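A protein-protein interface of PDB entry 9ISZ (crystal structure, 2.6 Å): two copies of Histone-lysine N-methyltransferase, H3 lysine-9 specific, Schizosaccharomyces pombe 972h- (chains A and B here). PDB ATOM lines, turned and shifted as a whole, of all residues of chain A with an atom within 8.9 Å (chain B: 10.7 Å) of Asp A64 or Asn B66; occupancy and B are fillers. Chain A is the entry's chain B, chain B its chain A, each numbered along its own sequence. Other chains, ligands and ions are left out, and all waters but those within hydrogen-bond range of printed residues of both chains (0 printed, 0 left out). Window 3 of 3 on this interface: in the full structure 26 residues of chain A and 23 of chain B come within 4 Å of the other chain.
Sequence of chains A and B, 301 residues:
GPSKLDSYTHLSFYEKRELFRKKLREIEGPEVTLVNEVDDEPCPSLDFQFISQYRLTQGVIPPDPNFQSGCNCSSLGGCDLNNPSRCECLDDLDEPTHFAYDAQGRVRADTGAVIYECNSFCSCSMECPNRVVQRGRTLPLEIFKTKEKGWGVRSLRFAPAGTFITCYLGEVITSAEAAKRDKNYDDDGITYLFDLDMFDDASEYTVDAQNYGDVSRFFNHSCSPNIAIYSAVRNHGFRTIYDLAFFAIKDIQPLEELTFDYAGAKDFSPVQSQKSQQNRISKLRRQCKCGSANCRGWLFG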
ATOM      1  N   ILE A  61      -0.047 -23.290  -1.211  1.00  0.00           N
ATOM      2  CA  ILE A  61      -0.283 -21.903  -1.602  1.00  0.00           C
ATOM      3  C   ILE A  61       0.825 -21.055  -0.986  1.00  0.00           C
ATOM      4  O   ILE A  61       1.057 -21.110   0.231  1.00  0.00           O
ATOM      5  CB  ILE A  61      -1.697 -21.428  -1.215  1.00  0.00           C
ATOM      6  CG1 ILE A  61      -2.024 -20.106  -1.911  1.00  0.00           C
ATOM      7  CG2 ILE A  61      -1.880 -21.305   0.295  1.00  0.00           C
ATOM      8  CD1 ILE A  61      -2.214 -20.239  -3.409  1.00  0.00           C
ATOM      9  N   PRO A  62       1.578 -20.316  -1.794  1.00  0.00           N
ATOM     10  CA  PRO A  62       2.674 -19.501  -1.258  1.00  0.00           C
ATOM     11  C   PRO A  62       2.147 -18.240  -0.598  1.00  0.00           C
ATOM     12  O   PRO A  62       0.978 -17.872  -0.790  1.00  0.00           O
ATOM     13  CB  PRO A  62       3.514 -19.176  -2.504  1.00  0.00           C
ATOM     14  CG  PRO A  62       2.580 -19.322  -3.643  1.00  0.00           C
ATOM     15  CD  PRO A  62       1.577 -20.363  -3.265  1.00  0.00           C
ATOM     16  N   PRO A  63       2.968 -17.559   0.202  1.00  0.00           N
ATOM     17  CA  PRO A  63       2.503 -16.330   0.856  1.00  0.00           C
ATOM     18  C   PRO A  63       2.053 -15.293  -0.163  1.00  0.00           C
ATOM     19  O   PRO A  63       2.749 -15.010  -1.140  1.00  0.00           O
ATOM     20  CB  PRO A  63       3.732 -15.858   1.641  1.00  0.00           C
ATOM     21  CG  PRO A  63       4.529 -17.101   1.868  1.00  0.00           C
ATOM     22  CD  PRO A  63       4.326 -17.933   0.638  1.00  0.00           C
ATOM     23  N   ASP A  64       0.873 -14.727   0.078  1.00  0.00           N
ATOM     24  CA  ASP A  64       0.309 -13.722  -0.808  1.00  0.00           C
ATOM     25  C   ASP A  64       0.835 -12.351  -0.410  1.00  0.00           C
ATOM     26  O   ASP A  64       0.604 -11.919   0.728  1.00  0.00           O
ATOM     27  CB  ASP A  64      -1.209 -13.744  -0.743  1.00  0.00           C
ATOM     28  CG  ASP A  64      -1.853 -12.807  -1.747  1.00  0.00           C
ATOM     29  OD1 ASP A  64      -1.118 -12.059  -2.428  1.00  0.00           O
ATOM     30  OD2 ASP A  64      -3.098 -12.817  -1.859  1.00  0.00           O
ATOM     31  N   PRO A  65       1.543 -11.643  -1.293  1.00  0.00           N
ATOM     32  CA  PRO A  65       2.091 -10.333  -0.914  1.00  0.00           C
ATOM     33  C   PRO A  65       1.035  -9.283  -0.623  1.00  0.00           C
ATOM     34  O   PRO A  65       1.356  -8.273   0.018  1.00  0.00           O
ATOM     35  CB  PRO A  65       2.937  -9.945  -2.132  1.00  0.00           C
ATOM     36  CG  PRO A  65       2.320 -10.692  -3.270  1.00  0.00           C
ATOM     37  CD  PRO A  65       1.857 -11.994  -2.689  1.00  0.00           C
ATOM     38  N   ASN A  66      -0.206  -9.475  -1.075  1.00  0.00           N
ATOM     39  CA  ASN A  66      -1.252  -8.496  -0.808  1.00  0.00           C
ATOM     40  C   ASN A  66      -1.608  -8.418   0.670  1.00  0.00           C
ATOM     41  O   ASN A  66      -2.136  -7.393   1.112  1.00  0.00           O
ATOM     42  CB  ASN A  66      -2.504  -8.821  -1.625  1.00  0.00           C
ATOM     43  CG  ASN A  66      -2.222  -8.902  -3.111  1.00  0.00           C
ATOM     44  OD1 ASN A  66      -2.278  -7.898  -3.822  1.00  0.00           O
ATOM     45  ND2 ASN A  66      -1.917 -10.105  -3.591  1.00  0.00           N
ATOM     46  N   PHE A  67      -1.337  -9.469   1.437  1.00  0.00           N
ATOM     47  CA  PHE A  67      -1.586  -9.477   2.871  1.00  0.00           C
ATOM     48  C   PHE A  67      -0.362  -9.055   3.673  1.00  0.00           C
ATOM     49  O   PHE A  67      -0.333  -9.246   4.894  1.00  0.00           O
ATOM     50  CB  PHE A  67      -2.057 -10.866   3.313  1.00  0.00           C
ATOM     51  CG  PHE A  67      -3.434 -11.229   2.817  1.00  0.00           C
ATOM     52  CD1 PHE A  67      -3.659 -11.490   1.473  1.00  0.00           C
ATOM     53  CD2 PHE A  67      -4.501 -11.316   3.696  1.00  0.00           C
ATOM     54  CE1 PHE A  67      -4.921 -11.819   1.017  1.00  0.00           C
ATOM     55  CE2 PHE A  67      -5.766 -11.648   3.245  1.00  0.00           C
ATOM     56  CZ  PHE A  67      -5.976 -11.900   1.903  1.00  0.00           C
ATOM     57  N   GLN A  68       0.643  -8.488   3.012  1.00  0.00           N
ATOM     58  CA  GLN A  68       1.889  -8.079   3.641  1.00  0.00           C
ATOM     59  C   GLN A  68       1.965  -6.559   3.688  1.00  0.00           C
ATOM     60  O   GLN A  68       1.632  -5.882   2.710  1.00  0.00           O
ATOM     61  CB  GLN A  68       3.089  -8.643   2.879  1.00  0.00           C
ATOM     62  CG  GLN A  68       4.426  -8.164   3.391  1.00  0.00           C
ATOM     63  CD  GLN A  68       5.574  -8.638   2.528  1.00  0.00           C
ATOM     64  OE1 GLN A  68       6.125  -9.718   2.748  1.00  0.00           O
ATOM     65  NE2 GLN A  68       5.940  -7.835   1.535  1.00  0.00           N
ATOM     66  N   SER A  69       2.395  -6.026   4.830  1.00  0.00           N
ATOM     67  CA  SER A  69       2.515  -4.589   5.026  1.00  0.00           C
ATOM     68  C   SER A  69       3.890  -4.266   5.593  1.00  0.00           C
ATOM     69  O   SER A  69       4.317  -4.870   6.583  1.00  0.00           O
ATOM     70  CB  SER A  69       1.421  -4.066   5.961  1.00  0.00           C
ATOM     71  OG  SER A  69       1.474  -4.718   7.217  1.00  0.00           O
ATOM     72  N   PHE A 121       8.336  -4.612   1.511  1.00  0.00           N
ATOM     73  CA  PHE A 121       7.527  -3.399   1.528  1.00  0.00           C
ATOM     74  C   PHE A 121       8.018  -2.356   2.525  1.00  0.00           C
ATOM     75  O   PHE A 121       7.483  -1.244   2.539  1.00  0.00           O
ATOM     76  CB  PHE A 121       6.065  -3.739   1.834  1.00  0.00           C
ATOM     77  CG  PHE A 121       5.383  -4.529   0.751  1.00  0.00           C
ATOM     78  CD1 PHE A 121       5.930  -4.609  -0.520  1.00  0.00           C
ATOM     79  CD2 PHE A 121       4.187  -5.183   1.002  1.00  0.00           C
ATOM     80  CE1 PHE A 121       5.300  -5.331  -1.518  1.00  0.00           C
ATOM     81  CE2 PHE A 121       3.553  -5.906   0.008  1.00  0.00           C
ATOM     82  CZ  PHE A 121       4.110  -5.979  -1.253  1.00  0.00           C
ATOM     83  N   ARG A 234       8.165 -12.842   7.502  1.00  0.00           N
ATOM     84  CA  ARG A 234       8.237 -11.587   6.764  1.00  0.00           C
ATOM     85  C   ARG A 234       6.870 -11.090   6.317  1.00  0.00           C
ATOM     86  O   ARG A 234       6.598  -9.888   6.390  1.00  0.00           O
ATOM     87  CB  ARG A 234       9.149 -11.731   5.545  1.00  0.00           C
ATOM     88  CG  ARG A 234      10.623 -11.593   5.865  1.00  0.00           C
ATOM     89  CD  ARG A 234      11.450 -11.514   4.595  1.00  0.00           C
ATOM     90  NE  ARG A 234      11.280 -12.703   3.771  1.00  0.00           N
ATOM     91  CZ  ARG A 234      11.964 -13.827   3.934  1.00  0.00           C
ATOM     92  NH1 ARG A 234      12.881 -13.947   4.880  1.00  0.00           N
ATOM     93  NH2 ARG A 234      11.722 -14.856   3.129  1.00  0.00           N
ATOM     94  N   ASN A 235       6.007 -11.991   5.850  1.00  0.00           N
ATOM     95  CA  ASN A 235       4.620 -11.661   5.537  1.00  0.00           C
ATOM     96  C   ASN A 235       3.807 -11.888   6.804  1.00  0.00           C
ATOM     97  O   ASN A 235       3.373 -13.008   7.083  1.00  0.00           O
ATOM     98  CB  ASN A 235       4.110 -12.509   4.376  1.00  0.00           C
ATOM     99  CG  ASN A 235       2.777 -12.019   3.835  1.00  0.00           C
ATOM    100  OD1 ASN A 235       2.059 -11.272   4.502  1.00  0.00           O
ATOM    101  ND2 ASN A 235       2.440 -12.439   2.620  1.00  0.00           N
ATOM    102  N   HIS A 236       3.595 -10.818   7.574  1.00  0.00           N
ATOM    103  CA  HIS A 236       2.947 -10.947   8.873  1.00  0.00           C
ATOM    104  C   HIS A 236       1.500 -11.403   8.767  1.00  0.00           C
ATOM    105  O   HIS A 236       0.952 -11.914   9.750  1.00  0.00           O
ATOM    106  CB  HIS A 236       3.024  -9.623   9.616  1.00  0.00           C
ATOM    107  CG  HIS A 236       4.361  -8.968   9.508  1.00  0.00           C
ATOM    108  ND1 HIS A 236       5.501  -9.518  10.051  1.00  0.00           N
ATOM    109  CD2 HIS A 236       4.749  -7.826   8.893  1.00  0.00           C
ATOM    110  CE1 HIS A 236       6.532  -8.735   9.789  1.00  0.00           C
ATOM    111  NE2 HIS A 236       6.103  -7.701   9.088  1.00  0.00           N
ATOM    112  N   GLY A 237       0.867 -11.229   7.605  1.00  0.00           N
ATOM    113  CA  GLY A 237      -0.484 -11.727   7.422  1.00  0.00           C
ATOM    114  C   GLY A 237      -0.574 -13.214   7.169  1.00  0.00           C
ATOM    115  O   GLY A 237      -1.659 -13.789   7.306  1.00  0.00           O
ATOM    116  N   PHE A 238       0.537 -13.850   6.808  1.00  0.00           N
ATOM    117  CA  PHE A 238       0.574 -15.274   6.511  1.00  0.00           C
ATOM    118  C   PHE A 238       1.225 -16.037   7.657  1.00  0.00           C
ATOM    119  O   PHE A 238       2.192 -15.564   8.261  1.00  0.00           O
ATOM    120  CB  PHE A 238       1.339 -15.541   5.215  1.00  0.00           C
ATOM    121  CG  PHE A 238       0.472 -16.012   4.085  1.00  0.00           C
ATOM    122  CD1 PHE A 238      -0.400 -15.139   3.453  1.00  0.00           C
ATOM    123  CD2 PHE A 238       0.536 -17.325   3.647  1.00  0.00           C
ATOM    124  CE1 PHE A 238      -1.196 -15.570   2.410  1.00  0.00           C
ATOM    125  CE2 PHE A 238      -0.257 -17.762   2.603  1.00  0.00           C
ATOM    126  CZ  PHE A 238      -1.124 -16.882   1.984  1.00  0.00           C
ATOM    127  N   ARG A 239       0.714 -17.226   7.918  1.00  0.00           N
ATOM    128  CA  ARG A 239       1.255 -18.057   8.980  1.00  0.00           C
ATOM    129  C   ARG A 239       1.295 -19.547   8.583  1.00  0.00           C
ATOM    130  O   ARG A 239       1.526 -20.397   9.427  1.00  0.00           O
ATOM    131  CB  ARG A 239       0.497 -17.825  10.286  1.00  0.00           C
ATOM    132  CG  ARG A 239       0.613 -16.417  10.847  1.00  0.00           C
ATOM    133  CD  ARG A 239       0.366 -16.376  12.347  1.00  0.00           C
ATOM    134  NE  ARG A 239      -0.931 -15.797  12.691  1.00  0.00           N
ATOM    135  CZ  ARG A 239      -1.211 -14.496  12.669  1.00  0.00           C
ATOM    136  NH1 ARG A 239      -0.290 -13.612  12.319  1.00  0.00           N
ATOM    137  NH2 ARG A 239      -2.421 -14.078  13.001  1.00  0.00           N
ATOM    138  N   THR A 240       1.031 -19.872   7.323  1.00  0.00           N
ATOM    139  CA  THR A 240       1.195 -21.236   6.841  1.00  0.00           C
ATOM    140  C   THR A 240       2.612 -21.508   6.361  1.00  0.00           C
ATOM    141  O   THR A 240       3.063 -22.660   6.394  1.00  0.00           O
ATOM    142  CB  THR A 240       0.206 -21.522   5.707  1.00  0.00           C
ATOM    143  OG1 THR A 240       0.220 -20.438   4.768  1.00  0.00           O
ATOM    144  CG2 THR A 240      -1.203 -21.698   6.254  1.00  0.00           C
ATOM    145  N   ILE A 241       3.319 -20.471   5.914  1.00  0.00           N
ATOM    146  CA  ILE A 241       4.691 -20.584   5.438  1.00  0.00           C
ATOM    147  C   ILE A 241       5.528 -19.522   6.138  1.00  0.00           C
ATOM    148  O   ILE A 241       5.159 -18.343   6.150  1.00  0.00           O
ATOM    149  CB  ILE A 241       4.781 -20.428   3.909  1.00  0.00           C
ATOM    150  CG1 ILE A 241       3.914 -21.485   3.218  1.00  0.00           C
ATOM    151  CG2 ILE A 241       6.226 -20.530   3.446  1.00  0.00           C
ATOM    152  CD1 ILE A 241       3.956 -21.423   1.711  1.00  0.00           C
ATOM    153  N   LEU B  56      13.406  -6.811  -3.879  1.00  0.00           N
ATOM    154  CA  LEU B  56      12.360  -5.840  -4.156  1.00  0.00           C
ATOM    155  C   LEU B  56      12.414  -4.695  -3.150  1.00  0.00           C
ATOM    156  O   LEU B  56      12.862  -4.859  -2.012  1.00  0.00           O
ATOM    157  CB  LEU B  56      10.989  -6.512  -4.117  1.00  0.00           C
ATOM    158  CG  LEU B  56      10.901  -7.855  -4.842  1.00  0.00           C
ATOM    159  CD1 LEU B  56       9.556  -8.510  -4.592  1.00  0.00           C
ATOM    160  CD2 LEU B  56      11.145  -7.679  -6.330  1.00  0.00           C
ATOM    161  N   ILE B  61       5.194  -3.770  -6.786  1.00  0.00           N
ATOM    162  CA  ILE B  61       4.179  -4.807  -6.613  1.00  0.00           C
ATOM    163  C   ILE B  61       4.753  -6.146  -7.063  1.00  0.00           C
ATOM    164  O   ILE B  61       4.991  -6.345  -8.263  1.00  0.00           O
ATOM    165  CB  ILE B  61       2.898  -4.466  -7.389  1.00  0.00           C
ATOM    166  CG1 ILE B  61       2.404  -3.066  -7.014  1.00  0.00           C
ATOM    167  CG2 ILE B  61       1.827  -5.513  -7.128  1.00  0.00           C
ATOM    168  CD1 ILE B  61       2.182  -2.871  -5.528  1.00  0.00           C
ATOM    169  N   PRO B  62       4.982  -7.084  -6.149  1.00  0.00           N
ATOM    170  CA  PRO B  62       5.582  -8.368  -6.527  1.00  0.00           C
ATOM    171  C   PRO B  62       4.556  -9.287  -7.164  1.00  0.00           C
ATOM    172  O   PRO B  62       3.344  -9.030  -7.085  1.00  0.00           O
ATOM    173  CB  PRO B  62       6.083  -8.925  -5.187  1.00  0.00           C
ATOM    174  CG  PRO B  62       5.187  -8.329  -4.182  1.00  0.00           C
ATOM    175  CD  PRO B  62       4.732  -6.993  -4.700  1.00  0.00           C
ATOM    176  N   PRO B  63       4.999 -10.364  -7.813  1.00  0.00           N
ATOM    177  CA  PRO B  63       4.048 -11.276  -8.470  1.00  0.00           C
ATOM    178  C   PRO B  63       3.039 -11.850  -7.486  1.00  0.00           C
ATOM    179  O   PRO B  63       3.399 -12.449  -6.470  1.00  0.00           O
ATOM    180  CB  PRO B  63       4.955 -12.369  -9.051  1.00  0.00           C
ATOM    181  CG  PRO B  63       6.282 -11.703  -9.230  1.00  0.00           C
ATOM    182  CD  PRO B  63       6.401 -10.732  -8.093  1.00  0.00           C
ATOM    183  N   ASP B  64       1.763 -11.659  -7.800  1.00  0.00           N
ATOM    184  CA  ASP B  64       0.692 -12.265  -7.022  1.00  0.00           C
ATOM    185  C   ASP B  64       0.579 -13.735  -7.404  1.00  0.00           C
ATOM    186  O   ASP B  64       0.296 -14.040  -8.570  1.00  0.00           O
ATOM    187  CB  ASP B  64      -0.626 -11.539  -7.282  1.00  0.00           C
ATOM    188  CG  ASP B  64      -1.712 -11.891  -6.278  1.00  0.00           C
ATOM    189  OD1 ASP B  64      -1.670 -12.996  -5.698  1.00  0.00           O
ATOM    190  OD2 ASP B  64      -2.620 -11.055  -6.078  1.00  0.00           O
ATOM    191  N   PRO B  65       0.790 -14.670  -6.474  1.00  0.00           N
ATOM    192  CA  PRO B  65       0.723 -16.094  -6.830  1.00  0.00           C
ATOM    193  C   PRO B  65      -0.679 -16.575  -7.145  1.00  0.00           C
ATOM    194  O   PRO B  65      -0.829 -17.680  -7.685  1.00  0.00           O
ATOM    195  CB  PRO B  65       1.277 -16.788  -5.584  1.00  0.00           C
ATOM    196  CG  PRO B  65       0.931 -15.859  -4.471  1.00  0.00           C
ATOM    197  CD  PRO B  65       1.083 -14.474  -5.044  1.00  0.00           C
ATOM    198  N   ASN B  66      -1.707 -15.792  -6.818  1.00  0.00           N
ATOM    199  CA  ASN B  66      -3.072 -16.175  -7.142  1.00  0.00           C
ATOM    200  C   ASN B  66      -3.320 -16.213  -8.644  1.00  0.00           C
ATOM    201  O   ASN B  66      -4.283 -16.851  -9.085  1.00  0.00           O
ATOM    202  CB  ASN B  66      -4.054 -15.212  -6.477  1.00  0.00           C
ATOM    203  CG  ASN B  66      -3.919 -15.189  -4.966  1.00  0.00           C
ATOM    204  OD1 ASN B  66      -4.275 -16.149  -4.284  1.00  0.00           O
ATOM    205  ND2 ASN B  66      -3.419 -14.079  -4.434  1.00  0.00           N
ATOM    206  N   PHE B  67      -2.477 -15.549  -9.438  1.00  0.00           N
ATOM    207  CA  PHE B  67      -2.595 -15.544 -10.890  1.00  0.00           C
ATOM    208  C   PHE B  67      -1.622 -16.513 -11.551  1.00  0.00           C
ATOM    209  O   PHE B  67      -1.360 -16.400 -12.754  1.00  0.00           O
ATOM    210  CB  PHE B  67      -2.385 -14.130 -11.432  1.00  0.00           C
ATOM    211  CG  PHE B  67      -3.490 -13.174 -11.081  1.00  0.00           C
ATOM    212  CD1 PHE B  67      -3.510 -12.535  -9.852  1.00  0.00           C
ATOM    213  CD2 PHE B  67      -4.508 -12.912 -11.984  1.00  0.00           C
ATOM    214  CE1 PHE B  67      -4.526 -11.653  -9.527  1.00  0.00           C
ATOM    215  CE2 PHE B  67      -5.523 -12.031 -11.666  1.00  0.00           C
ATOM    216  CZ  PHE B  67      -5.533 -11.402 -10.435  1.00  0.00           C
ATOM    217  N   GLN B  68      -1.084 -17.460 -10.789  1.00  0.00           N
ATOM    218  CA  GLN B  68      -0.087 -18.399 -11.275  1.00  0.00           C
ATOM    219  C   GLN B  68      -0.687 -19.796 -11.335  1.00  0.00           C
ATOM    220  O   GLN B  68      -1.457 -20.190 -10.454  1.00  0.00           O
ATOM    221  CB  GLN B  68       1.148 -18.391 -10.371  1.00  0.00           C
ATOM    222  CG  GLN B  68       2.322 -19.182 -10.907  1.00  0.00           C
ATOM    223  CD  GLN B  68       3.494 -19.180  -9.951  1.00  0.00           C
ATOM    224  OE1 GLN B  68       4.599 -18.769 -10.306  1.00  0.00           O
ATOM    225  NE2 GLN B  68       3.259 -19.637  -8.728  1.00  0.00           N
ATOM    226  N   SER B  69      -0.341 -20.537 -12.386  1.00  0.00           N
ATOM    227  CA  SER B  69      -0.871 -21.876 -12.596  1.00  0.00           C
ATOM    228  C   SER B  69       0.247 -22.797 -13.059  1.00  0.00           C
ATOM    229  O   SER B  69       1.066 -22.424 -13.903  1.00  0.00           O
ATOM    230  CB  SER B  69      -2.013 -21.868 -13.620  1.00  0.00           C
ATOM    231  OG  SER B  69      -1.656 -21.125 -14.772  1.00  0.00           O
ATOM    232  N   GLY B  70       0.274 -24.004 -12.505  1.00  0.00           N
ATOM    233  CA  GLY B  70       1.304 -24.978 -12.813  1.00  0.00           C
ATOM    234  C   GLY B  70       0.774 -26.102 -13.683  1.00  0.00           C
ATOM    235  O   GLY B  70      -0.422 -26.413 -13.663  1.00  0.00           O
ATOM    236  N   ASN B 119       6.731 -23.598 -12.244  1.00  0.00           N
ATOM    237  CA  ASN B 119       6.679 -22.900 -10.968  1.00  0.00           C
ATOM    238  C   ASN B 119       6.354 -23.900  -9.860  1.00  0.00           C
ATOM    239  O   ASN B 119       6.360 -25.115 -10.071  1.00  0.00           O
ATOM    240  CB  ASN B 119       5.634 -21.784 -11.015  1.00  0.00           C
ATOM    241  CG  ASN B 119       4.335 -22.231 -11.649  1.00  0.00           C
ATOM    242  OD1 ASN B 119       3.604 -23.045 -11.084  1.00  0.00           O
ATOM    243  ND2 ASN B 119       4.038 -21.699 -12.830  1.00  0.00           N
ATOM    244  N   SER B 120       6.108 -23.370  -8.658  1.00  0.00           N
ATOM    245  CA  SER B 120       5.738 -24.216  -7.527  1.00  0.00           C
ATOM    246  C   SER B 120       4.471 -25.027  -7.776  1.00  0.00           C
ATOM    247  O   SER B 120       4.333 -26.140  -7.253  1.00  0.00           O
ATOM    248  CB  SER B 120       5.568 -23.363  -6.272  1.00  0.00           C
ATOM    249  OG  SER B 120       5.189 -24.166  -5.163  1.00  0.00           O
ATOM    250  N   PHE B 121       3.536 -24.495  -8.555  1.00  0.00           N
ATOM    251  CA  PHE B 121       2.279 -25.196  -8.771  1.00  0.00           C
ATOM    252  C   PHE B 121       2.411 -26.383  -9.715  1.00  0.00           C
ATOM    253  O   PHE B 121       1.497 -27.213  -9.767  1.00  0.00           O
ATOM    254  CB  PHE B 121       1.224 -24.217  -9.289  1.00  0.00           C
ATOM    255  CG  PHE B 121       0.936 -23.094  -8.339  1.00  0.00           C
ATOM    256  CD1 PHE B 121       1.026 -23.292  -6.971  1.00  0.00           C
ATOM    257  CD2 PHE B 121       0.588 -21.840  -8.809  1.00  0.00           C
ATOM    258  CE1 PHE B 121       0.764 -22.264  -6.091  1.00  0.00           C
ATOM    259  CE2 PHE B 121       0.326 -20.808  -7.933  1.00  0.00           C
ATOM    260  CZ  PHE B 121       0.415 -21.020  -6.572  1.00  0.00           C
ATOM    261  N   ARG B 234       8.143 -17.383 -14.327  1.00  0.00           N
ATOM    262  CA  ARG B 234       7.585 -18.462 -13.525  1.00  0.00           C
ATOM    263  C   ARG B 234       6.123 -18.247 -13.173  1.00  0.00           C
ATOM    264  O   ARG B 234       5.373 -19.221 -13.081  1.00  0.00           O
ATOM    265  CB  ARG B 234       8.401 -18.654 -12.239  1.00  0.00           C
ATOM    266  CG  ARG B 234       9.685 -19.447 -12.458  1.00  0.00           C
ATOM    267  CD  ARG B 234      10.487 -19.632 -11.176  1.00  0.00           C
ATOM    268  NE  ARG B 234      11.182 -18.416 -10.776  1.00  0.00           N
ATOM    269  CZ  ARG B 234      10.760 -17.586  -9.833  1.00  0.00           C
ATOM    270  NH1 ARG B 234       9.646 -17.816  -9.159  1.00  0.00           N
ATOM    271  NH2 ARG B 234      11.474 -16.499  -9.558  1.00  0.00           N
ATOM    272  N   ASN B 235       5.702 -17.002 -12.979  1.00  0.00           N
ATOM    273  CA  ASN B 235       4.287 -16.651 -12.915  1.00  0.00           C
ATOM    274  C   ASN B 235       3.919 -16.109 -14.291  1.00  0.00           C
ATOM    275  O   ASN B 235       4.123 -14.928 -14.579  1.00  0.00           O
ATOM    276  CB  ASN B 235       4.012 -15.632 -11.814  1.00  0.00           C
ATOM    277  CG  ASN B 235       2.527 -15.391 -11.596  1.00  0.00           C
ATOM    278  OD1 ASN B 235       1.693 -15.812 -12.397  1.00  0.00           O
ATOM    279  ND2 ASN B 235       2.194 -14.705 -10.508  1.00  0.00           N
ATOM    280  N   HIS B 236       3.373 -16.981 -15.140  1.00  0.00           N
ATOM    281  CA  HIS B 236       3.108 -16.603 -16.524  1.00  0.00           C
ATOM    282  C   HIS B 236       2.097 -15.466 -16.625  1.00  0.00           C
ATOM    283  O   HIS B 236       2.094 -14.725 -17.614  1.00  0.00           O
ATOM    284  CB  HIS B 236       2.622 -17.822 -17.302  1.00  0.00           C
ATOM    285  CG  HIS B 236       3.343 -19.086 -16.948  1.00  0.00           C
ATOM    286  ND1 HIS B 236       4.507 -19.478 -17.572  1.00  0.00           N
ATOM    287  CD2 HIS B 236       3.069 -20.039 -16.026  1.00  0.00           C
ATOM    288  CE1 HIS B 236       4.917 -20.622 -17.053  1.00  0.00           C
ATOM    289  NE2 HIS B 236       4.062 -20.983 -16.113  1.00  0.00           N
ATOM    290  N   GLY B 237       1.230 -15.312 -15.620  1.00  0.00           N
ATOM    291  CA  GLY B 237       0.264 -14.226 -15.656  1.00  0.00           C
ATOM    292  C   GLY B 237       0.910 -12.855 -15.565  1.00  0.00           C
ATOM    293  O   GLY B 237       0.562 -11.943 -16.321  1.00  0.00           O
ATOM    294  N   PHE B 238       1.863 -12.693 -14.652  1.00  0.00           N
ATOM    295  CA  PHE B 238       2.514 -11.410 -14.428  1.00  0.00           C
ATOM    296  C   PHE B 238       3.669 -11.199 -15.395  1.00  0.00           C
ATOM    297  O   PHE B 238       4.372 -12.136 -15.773  1.00  0.00           O
ATOM    298  CB  PHE B 238       3.027 -11.299 -12.994  1.00  0.00           C
ATOM    299  CG  PHE B 238       2.038 -10.691 -12.052  1.00  0.00           C
ATOM    300  CD1 PHE B 238       1.974  -9.317 -11.885  1.00  0.00           C
ATOM    301  CD2 PHE B 238       1.160 -11.489 -11.344  1.00  0.00           C
ATOM    302  CE1 PHE B 238       1.056  -8.752 -11.021  1.00  0.00           C
ATOM    303  CE2 PHE B 238       0.243 -10.933 -10.483  1.00  0.00           C
ATOM    304  CZ  PHE B 238       0.189  -9.562 -10.318  1.00  0.00           C
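The side-chain carboxylate (OD2) of Asp B64 is in hydrogen-bond range of the side-chain amide nitrogen (ND2) of Asn A66. The side-chain amide nitrogen (ND2) of Asn B66 lies within hydrogen-bond range of the side-chain carboxylate (OD2) of Asp A64 (2.9 Å). The side-chain carboxylate (OD1) of Asp A64 sits close to the side-chain carboxylate (OD1) of Asp B64.
OD1 of Asp B64 lies within hydrogen-bond range of ND2 of Asn B66 (2.4 Å). The backbone carbonyl oxygen of Asp B64 is in hydrogen-bond range of the side-chain amide nitrogen of Asn B235 (2.8 Å). N of Phe B121 lies within hydrogen-bond range of OD1 of Asn B119, 2.9 Å away. OD1 of Asp A64 sits at hydrogen-bond distance from ND2 of Asn A66 (2.4 Å). The backbone carbonyl oxygen of Asp A64 is in hydrogen-bond range of the side-chain amide nitrogen of Asn A235, 2.7 Å away.
Among the printed residues, merely in contact across the chains: Pro A62 with Pro B65, Pro A62 with Phe B121, Pro A63 with Pro B65, Pro A65 with Pro B62, Pro A65 with Pro B63, Pro A65 with Pro B65 and Phe A121 with Pro B62.
Asp A64 touches two residues of chain B. Asn B66 touches one residue of chain A. Pro A63 touches just one residue of chain B: Pro B65. Pro A65 touches three residues of chain B. Asn A66 touches just one residue of chain B: Asp B64 (2.8 Å). No residue of chain B comes within 4 Å of Phe A67. Printed residues of chain A within 4 Å of Pro B62: Pro A65 and Phe A121. Of the printed residues of chain A, Phe B121 touches Pro A62. Gly A237 touches none of the printed residues of chain B. Arg A239 touches none of the printed residues of chain B.
Of the 18 printed residues of chain A, 6 touch a printed residue of chain B. Of the 19 printed residues of chain B, 6 touch a printed residue of chain A.
Pro A62 touches Pro B65, and with the chains exchanged Pro A65 touches Pro B62. Pro A62 touches Phe B121, and with the chains exchanged Phe A121 touches Pro B62. Pro A63 touches Pro B65, and with the chains exchanged Pro A65 touches Pro B63. Pro A65 touches its own counterpart, Pro B65. 15 positions are printed for both chains. Of the 10 pairs that touch across the chains among the printed residues, 10 have their exchanged pair printed and touching as well.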
